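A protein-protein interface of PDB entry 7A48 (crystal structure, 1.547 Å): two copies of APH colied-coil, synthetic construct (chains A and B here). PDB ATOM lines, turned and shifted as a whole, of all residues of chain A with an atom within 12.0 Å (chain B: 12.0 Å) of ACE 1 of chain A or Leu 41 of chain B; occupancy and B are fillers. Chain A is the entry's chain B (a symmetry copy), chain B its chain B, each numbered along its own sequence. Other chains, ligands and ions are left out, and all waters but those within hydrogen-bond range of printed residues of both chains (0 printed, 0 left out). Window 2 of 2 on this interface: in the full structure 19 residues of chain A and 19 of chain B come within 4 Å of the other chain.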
ATOM      1  C   ACE A   1      -8.726 -27.635   5.489  1.00  0.00           C
ATOM      2  O   ACE A   1      -9.486 -27.297   6.394  1.00  0.00           O
ATOM      3  CH3 ACE A   1      -8.805 -26.963   4.128  1.00  0.00           C
ATOM      4  N   LEU A   2      -7.798 -28.575   5.649  1.00  0.00           N
ATOM      5  CA  LEU A   2      -7.785 -29.377   6.859  1.00  0.00           C
ATOM      6  C   LEU A   2      -6.359 -29.660   7.314  1.00  0.00           C
ATOM      7  O   LEU A   2      -5.378 -29.092   6.810  1.00  0.00           O
ATOM      8  CB  LEU A   2      -8.571 -30.679   6.658  1.00  0.00           C
ATOM      9  CG  LEU A   2      -8.527 -31.566   5.419  1.00  0.00           C
ATOM     10  CD1 LEU A   2      -7.166 -32.050   5.111  1.00  0.00           C
ATOM     11  CD2 LEU A   2      -9.404 -32.757   5.685  1.00  0.00           C
ATOM     12  N   GLU A   3      -6.285 -30.554   8.302  1.00  0.00           N
ATOM     13  CA  GLU A   3      -5.028 -30.942   8.929  1.00  0.00           C
ATOM     14  C   GLU A   3      -4.058 -31.510   7.903  1.00  0.00           C
ATOM     15  O   GLU A   3      -2.909 -31.066   7.800  1.00  0.00           O
ATOM     16  CB  GLU A   3      -5.328 -31.969  10.024  1.00  0.00           C
ATOM     17  CG  GLU A   3      -4.140 -32.631  10.697  1.00  0.00           C
ATOM     18  CD  GLU A   3      -4.463 -33.085  12.122  1.00  0.00           C
ATOM     19  OE1 GLU A   3      -3.884 -34.102  12.555  1.00  0.00           O
ATOM     20  OE2 GLU A   3      -5.297 -32.440  12.804  1.00  0.00           O
ATOM     21  N   GLU A   4      -4.512 -32.482   7.115  1.00  0.00           N
ATOM     22  CA  GLU A   4      -3.626 -33.179   6.189  1.00  0.00           C
ATOM     23  C   GLU A   4      -3.252 -32.308   5.001  1.00  0.00           C
ATOM     24  O   GLU A   4      -2.110 -32.356   4.529  1.00  0.00           O
ATOM     25  CB  GLU A   4      -4.278 -34.475   5.715  1.00  0.00           C
ATOM     26  CG  GLU A   4      -3.632 -35.707   6.313  1.00  0.00           C
ATOM     27  CD  GLU A   4      -2.118 -35.614   6.307  1.00  0.00           C
ATOM     28  OE1 GLU A   4      -1.542 -35.484   5.204  1.00  0.00           O
ATOM     29  OE2 GLU A   4      -1.503 -35.674   7.394  1.00  0.00           O
ATOM     30  N   GLU A   5      -4.199 -31.514   4.505  1.00  0.00           N
ATOM     31  CA  GLU A   5      -3.888 -30.569   3.442  1.00  0.00           C
ATOM     32  C   GLU A   5      -2.820 -29.586   3.891  1.00  0.00           C
ATOM     33  O   GLU A   5      -1.875 -29.306   3.145  1.00  0.00           O
ATOM     34  CB  GLU A   5      -5.153 -29.832   3.002  1.00  0.00           C
ATOM     35  CG  GLU A   5      -4.971 -29.001   1.746  1.00  0.00           C
ATOM     36  CD  GLU A   5      -6.271 -28.788   0.992  1.00  0.00           C
ATOM     37  OE1 GLU A   5      -6.219 -28.246  -0.134  1.00  0.00           O
ATOM     38  OE2 GLU A   5      -7.341 -29.161   1.522  1.00  0.00           O
ATOM     39  N   LEU A   6      -2.939 -29.066   5.119  1.00  0.00           N
ATOM     40  CA  LEU A   6      -1.956 -28.092   5.598  1.00  0.00           C
ATOM     41  C   LEU A   6      -0.596 -28.743   5.803  1.00  0.00           C
ATOM     42  O   LEU A   6       0.437 -28.160   5.458  1.00  0.00           O
ATOM     43  CB  LEU A   6      -2.432 -27.455   6.903  1.00  0.00           C
ATOM     44  CG  LEU A   6      -3.543 -26.408   6.870  1.00  0.00           C
ATOM     45  CD1 LEU A   6      -4.105 -26.242   8.275  1.00  0.00           C
ATOM     46  CD2 LEU A   6      -3.037 -25.086   6.332  1.00  0.00           C
ATOM     47  N   LYS A   7      -0.586 -29.945   6.356  1.00  0.00           N
ATOM     48  CA  LYS A   7       0.665 -30.618   6.624  1.00  0.00           C
ATOM     49  C   LYS A   7       1.409 -30.985   5.357  1.00  0.00           C
ATOM     50  O   LYS A   7       2.608 -30.768   5.254  1.00  0.00           O
ATOM     51  CB  LYS A   7       0.441 -31.871   7.471  1.00  0.00           C
ATOM     52  CG  LYS A   7       1.572 -32.871   7.368  1.00  0.00           C
ATOM     53  CD  LYS A   7       1.813 -33.593   8.682  1.00  0.00           C
ATOM     54  CE  LYS A   7       3.213 -34.188   8.729  1.00  0.00           C
ATOM     55  NZ  LYS A   7       4.266 -33.146   8.592  1.00  0.00           N
ATOM     56  N   GLN A   8       0.693 -31.527   4.387  1.00  0.00           N
ATOM     57  CA  GLN A   8       1.322 -31.946   3.140  1.00  0.00           C
ATOM     58  C   GLN A   8       1.800 -30.748   2.326  1.00  0.00           C
ATOM     59  O   GLN A   8       2.921 -30.759   1.803  1.00  0.00           O
ATOM     60  CB  GLN A   8       0.344 -32.803   2.339  1.00  0.00           C
ATOM     61  CG  GLN A   8       0.972 -33.641   1.246  1.00  0.00           C
ATOM     62  CD  GLN A   8       0.068 -34.775   0.773  1.00  0.00           C
ATOM     63  OE1 GLN A   8      -0.962 -35.075   1.387  1.00  0.00           O
ATOM     64  NE2 GLN A   8       0.457 -35.413  -0.328  1.00  0.00           N
ATOM     65  N   LEU A   9       0.968 -29.707   2.200  1.00  0.00           N
ATOM     66  CA  LEU A   9       1.381 -28.517   1.458  1.00  0.00           C
ATOM     67  C   LEU A   9       2.579 -27.841   2.122  1.00  0.00           C
ATOM     68  O   LEU A   9       3.453 -27.292   1.440  1.00  0.00           O
ATOM     69  CB  LEU A   9       0.206 -27.541   1.339  1.00  0.00           C
ATOM     70  CG  LEU A   9       0.467 -26.259   0.544  1.00  0.00           C
ATOM     71  CD1 LEU A   9       1.010 -26.575  -0.846  1.00  0.00           C
ATOM     72  CD2 LEU A   9      -0.798 -25.439   0.451  1.00  0.00           C
ATOM     73  N   GLU A  10       2.635 -27.876   3.453  1.00  0.00           N
ATOM     74  CA  GLU A  10       3.806 -27.363   4.158  1.00  0.00           C
ATOM     75  C   GLU A  10       5.062 -28.125   3.758  1.00  0.00           C
ATOM     76  O   GLU A  10       6.120 -27.521   3.531  1.00  0.00           O
ATOM     77  CB  GLU A  10       3.580 -27.441   5.671  1.00  0.00           C
ATOM     78  CG  GLU A  10       4.804 -27.141   6.527  1.00  0.00           C
ATOM     79  CD  GLU A  10       5.204 -25.687   6.480  1.00  0.00           C
ATOM     80  OE1 GLU A  10       4.441 -24.892   5.906  1.00  0.00           O
ATOM     81  OE2 GLU A  10       6.279 -25.337   7.015  1.00  0.00           O
ATOM     82  N   ARG B  30       2.455 -20.764  -2.457  1.00  0.00           N
ATOM     83  CA  ARG B  30       2.039 -21.792  -1.534  1.00  0.00           C
ATOM     84  C   ARG B  30       1.855 -21.245  -0.134  1.00  0.00           C
ATOM     85  O   ARG B  30       0.997 -21.702   0.594  1.00  0.00           O
ATOM     86  CB  ARG B  30       3.008 -22.967  -1.575  1.00  0.00           C
ATOM     87  CG  ARG B  30       2.823 -23.788  -2.832  1.00  0.00           C
ATOM     88  CD  ARG B  30       4.080 -24.499  -3.261  1.00  0.00           C
ATOM     89  NE  ARG B  30       3.833 -25.319  -4.432  1.00  0.00           N
ATOM     90  CZ  ARG B  30       3.786 -24.859  -5.674  1.00  0.00           C
ATOM     91  NH1 ARG B  30       3.973 -23.576  -5.924  1.00  0.00           N
ATOM     92  NH2 ARG B  30       3.555 -25.693  -6.666  1.00  0.00           N
ATOM     93  N   GLU B  32       0.720 -18.367   0.544  1.00  0.00           N
ATOM     94  CA  GLU B  32      -0.582 -17.717   0.504  1.00  0.00           C
ATOM     95  C   GLU B  32      -1.703 -18.738   0.568  1.00  0.00           C
ATOM     96  O   GLU B  32      -2.739 -18.489   1.193  1.00  0.00           O
ATOM     97  CB  GLU B  32      -0.684 -16.864  -0.763  1.00  0.00           C
ATOM     98  CG  GLU B  32       0.158 -15.590  -0.668  1.00  0.00           C
ATOM     99  CD  GLU B  32       0.269 -14.859  -1.985  1.00  0.00           C
ATOM    100  OE1 GLU B  32      -0.420 -15.278  -2.938  1.00  0.00           O
ATOM    101  OE2 GLU B  32       1.023 -13.860  -2.042  1.00  0.00           O
ATOM    102  N   LYS B  33      -1.516 -19.892  -0.064  1.00  0.00           N
ATOM    103  CA  LYS B  33      -2.532 -20.935   0.016  1.00  0.00           C
ATOM    104  C   LYS B  33      -2.651 -21.459   1.443  1.00  0.00           C
ATOM    105  O   LYS B  33      -3.765 -21.648   1.953  1.00  0.00           O
ATOM    106  CB  LYS B  33      -2.191 -22.061  -0.961  1.00  0.00           C
ATOM    107  CG  LYS B  33      -3.207 -23.195  -1.012  1.00  0.00           C
ATOM    108  CD  LYS B  33      -4.590 -22.694  -1.376  1.00  0.00           C
ATOM    109  CE  LYS B  33      -5.523 -23.851  -1.709  1.00  0.00           C
ATOM    110  NZ  LYS B  33      -6.889 -23.643  -1.156  1.00  0.00           N
ATOM    111  N   LEU B  34      -1.514 -21.657   2.111  1.00  0.00           N
ATOM    112  CA  LEU B  34      -1.518 -22.140   3.494  1.00  0.00           C
ATOM    113  C   LEU B  34      -2.227 -21.156   4.413  1.00  0.00           C
ATOM    114  O   LEU B  34      -2.959 -21.561   5.328  1.00  0.00           O
ATOM    115  CB  LEU B  34      -0.083 -22.393   3.964  1.00  0.00           C
ATOM    116  CG  LEU B  34       0.567 -23.651   3.391  1.00  0.00           C
ATOM    117  CD1 LEU B  34       2.089 -23.608   3.528  1.00  0.00           C
ATOM    118  CD2 LEU B  34      -0.004 -24.884   4.067  1.00  0.00           C
ATOM    119  N   ALA B  35      -2.025 -19.856   4.182  1.00  0.00           N
ATOM    120  CA  ALA B  35      -2.723 -18.839   4.963  1.00  0.00           C
ATOM    121  C   ALA B  35      -4.226 -18.917   4.747  1.00  0.00           C
ATOM    122  O   ALA B  35      -5.007 -18.795   5.699  1.00  0.00           O
ATOM    123  CB  ALA B  35      -2.206 -17.449   4.588  1.00  0.00           C
ATOM    124  N   GLN B  36      -4.649 -19.115   3.496  1.00  0.00           N
ATOM    125  CA  GLN B  36      -6.074 -19.194   3.193  1.00  0.00           C
ATOM    126  C   GLN B  36      -6.708 -20.417   3.843  1.00  0.00           C
ATOM    127  O   GLN B  36      -7.804 -20.326   4.409  1.00  0.00           O
ATOM    128  CB  GLN B  36      -6.283 -19.207   1.679  1.00  0.00           C
ATOM    129  CG  GLN B  36      -7.676 -19.623   1.247  1.00  0.00           C
ATOM    130  CD  GLN B  36      -7.854 -19.553  -0.250  1.00  0.00           C
ATOM    131  OE1 GLN B  36      -7.865 -18.470  -0.838  1.00  0.00           O
ATOM    132  NE2 GLN B  36      -7.985 -20.713  -0.880  1.00  0.00           N
ATOM    133  N   LEU B  37      -6.039 -21.570   3.779  1.00  0.00           N
ATOM    134  CA  LEU B  37      -6.555 -22.763   4.447  1.00  0.00           C
ATOM    135  C   LEU B  37      -6.626 -22.566   5.959  1.00  0.00           C
ATOM    136  O   LEU B  37      -7.557 -23.060   6.618  1.00  0.00           O
ATOM    137  CB  LEU B  37      -5.686 -23.973   4.105  1.00  0.00           C
ATOM    138  CG  LEU B  37      -5.555 -24.359   2.632  1.00  0.00           C
ATOM    139  CD1 LEU B  37      -4.451 -25.403   2.487  1.00  0.00           C
ATOM    140  CD2 LEU B  37      -6.872 -24.882   2.070  1.00  0.00           C
ATOM    141  N   LYS B  38      -5.656 -21.840   6.523  1.00  0.00           N
ATOM    142  CA  LYS B  38      -5.669 -21.524   7.948  1.00  0.00           C
ATOM    143  C   LYS B  38      -6.925 -20.752   8.337  1.00  0.00           C
ATOM    144  O   LYS B  38      -7.458 -20.930   9.440  1.00  0.00           O
ATOM    145  CB  LYS B  38      -4.410 -20.730   8.303  1.00  0.00           C
ATOM    146  CG  LYS B  38      -4.425 -20.066   9.671  1.00  0.00           C
ATOM    147  CD  LYS B  38      -3.492 -18.858   9.709  1.00  0.00           C
ATOM    148  CE  LYS B  38      -2.080 -19.218   9.252  1.00  0.00           C
ATOM    149  NZ  LYS B  38      -1.279 -18.026   8.849  1.00  0.00           N
ATOM    150  N   GLU B  39      -7.425 -19.896   7.441  1.00  0.00           N
ATOM    151  CA  GLU B  39      -8.604 -19.098   7.750  1.00  0.00           C
ATOM    152  C   GLU B  39      -9.874 -19.936   7.718  1.00  0.00           C
ATOM    153  O   GLU B  39     -10.849 -19.598   8.394  1.00  0.00           O
ATOM    154  CB  GLU B  39      -8.720 -17.924   6.777  1.00  0.00           C
ATOM    155  CG  GLU B  39      -7.543 -16.958   6.816  1.00  0.00           C
ATOM    156  CD  GLU B  39      -7.221 -16.480   8.220  1.00  0.00           C
ATOM    157  OE1 GLU B  39      -6.280 -17.026   8.835  1.00  0.00           O
ATOM    158  OE2 GLU B  39      -7.908 -15.557   8.709  1.00  0.00           O
ATOM    159  N   LYS B  40      -9.883 -21.019   6.936  1.00  0.00           N
ATOM    160  CA  LYS B  40     -11.031 -21.917   6.883  1.00  0.00           C
ATOM    161  C   LYS B  40     -11.206 -22.711   8.170  1.00  0.00           C
ATOM    162  O   LYS B  40     -12.324 -23.148   8.471  1.00  0.00           O
ATOM    163  CB  LYS B  40     -10.895 -22.869   5.692  1.00  0.00           C
ATOM    164  CG  LYS B  40     -10.635 -22.147   4.375  1.00  0.00           C
ATOM    165  CD  LYS B  40     -10.759 -23.059   3.165  1.00  0.00           C
ATOM    166  CE  LYS B  40     -11.112 -22.245   1.920  1.00  0.00           C
ATOM    167  NZ  LYS B  40     -10.606 -22.847   0.653  1.00  0.00           N
ATOM    168  N   LEU B  41     -10.137 -22.904   8.934  1.00  0.00           N
ATOM    169  CA  LEU B  41     -10.225 -23.609  10.205  1.00  0.00           C
ATOM    170  C   LEU B  41     -10.782 -22.706  11.303  1.00  0.00           C
ATOM    171  O   LEU B  41     -11.505 -23.163  12.187  1.00  0.00           O
ATOM    172  CB  LEU B  41      -8.853 -24.151  10.605  1.00  0.00           C
ATOM    173  CG  LEU B  41      -8.395 -25.365   9.795  1.00  0.00           C
ATOM    174  CD1 LEU B  41      -7.134 -25.978  10.389  1.00  0.00           C
ATOM    175  CD2 LEU B  41      -9.520 -26.391   9.724  1.00  0.00           C
ATOM    176  N   NH2 B  42     -10.443 -21.421  11.238  1.00  0.00           N
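NZ of Lys 33 of chain B lies close to NE2 of Gln 36 of chain B, at 3.1 Å.
Among the printed residues, pairs that only touch across the chains: ACE 1 of chain A with Leu 41 of chain B, ACE 1 of chain A with Leu 37 of chain B, Glu 10 of chain A with Leu 34 of chain B, Leu 6 of chain A with Leu 34 of chain B, Leu 9 of chain A with Lys 33 of chain B, Leu 6 of chain A with Leu 37 of chain B, Leu 9 of chain A with Leu 34 of chain B, Leu 6 of chain A with Leu 41 of chain B, Glu 5 of chain A with Leu 37 of chain B and Leu 9 of chain A with Arg 30 of chain B.
Of chain B, only Leu 37 and Leu 41 come within 4 Å of ACE 1 of chain A.
Of the printed residues of chain B, Glu 5 of chain A touches Leu 37 (3.7 Å).
Leu 37 of chain B touches just these residues of chain A: ACE 1, Glu 5 and Leu 6.
No residue of chain A comes within 4 Å of Glu 39 of chain B.
No residue of chain A comes within 4 Å of Lys 40 of chain B.
No residue of chain A comes within 4 Å of NH2 42 of chain B.
Printed residues of chain A within 4 Å of Leu 34 of chain B: Leu 6 (3.6 Å), Leu 9 (3.7 Å) and Glu 10 (3.6 Å).
Printed residues of chain B within 4 Å of Glu 10 of chain A: Leu 34.
Of the printed residues of chain A, Arg 30 of chain B touches Leu 9 (3.9 Å).
Gln 36 of chain B touches none of the printed residues of chain A.
Glu 32 of chain B touches none of the printed residues of chain A.
The nearest printed residue of chain B that does not touch Leu 9 of chain A is Leu 37 of chain B (4.2 Å).
Of the 10 printed residues of chain A, 5 touch a printed residue of chain B.
Printed residues of chain A that touch a printed residue of chain B: ACE 1, Glu 5, Leu 6, Leu 9 and Glu 10.
Hydrophobic or aromatic side chains of chain A within 4 Å of the printed part of chain B: Leu 6 and Leu 9.
Hydrophobic or aromatic side chains of chain B within 4 Å of the printed part of chain A: Leu 34, Leu 37 and Leu 41.
Among the printed residues, 10 pairs touch across the chains.
Among the printed residues, no Asp or Glu carboxylate lies within 4 Å of a Lys or Arg side-chain nitrogen of the other chain.
No position is printed for both chains.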
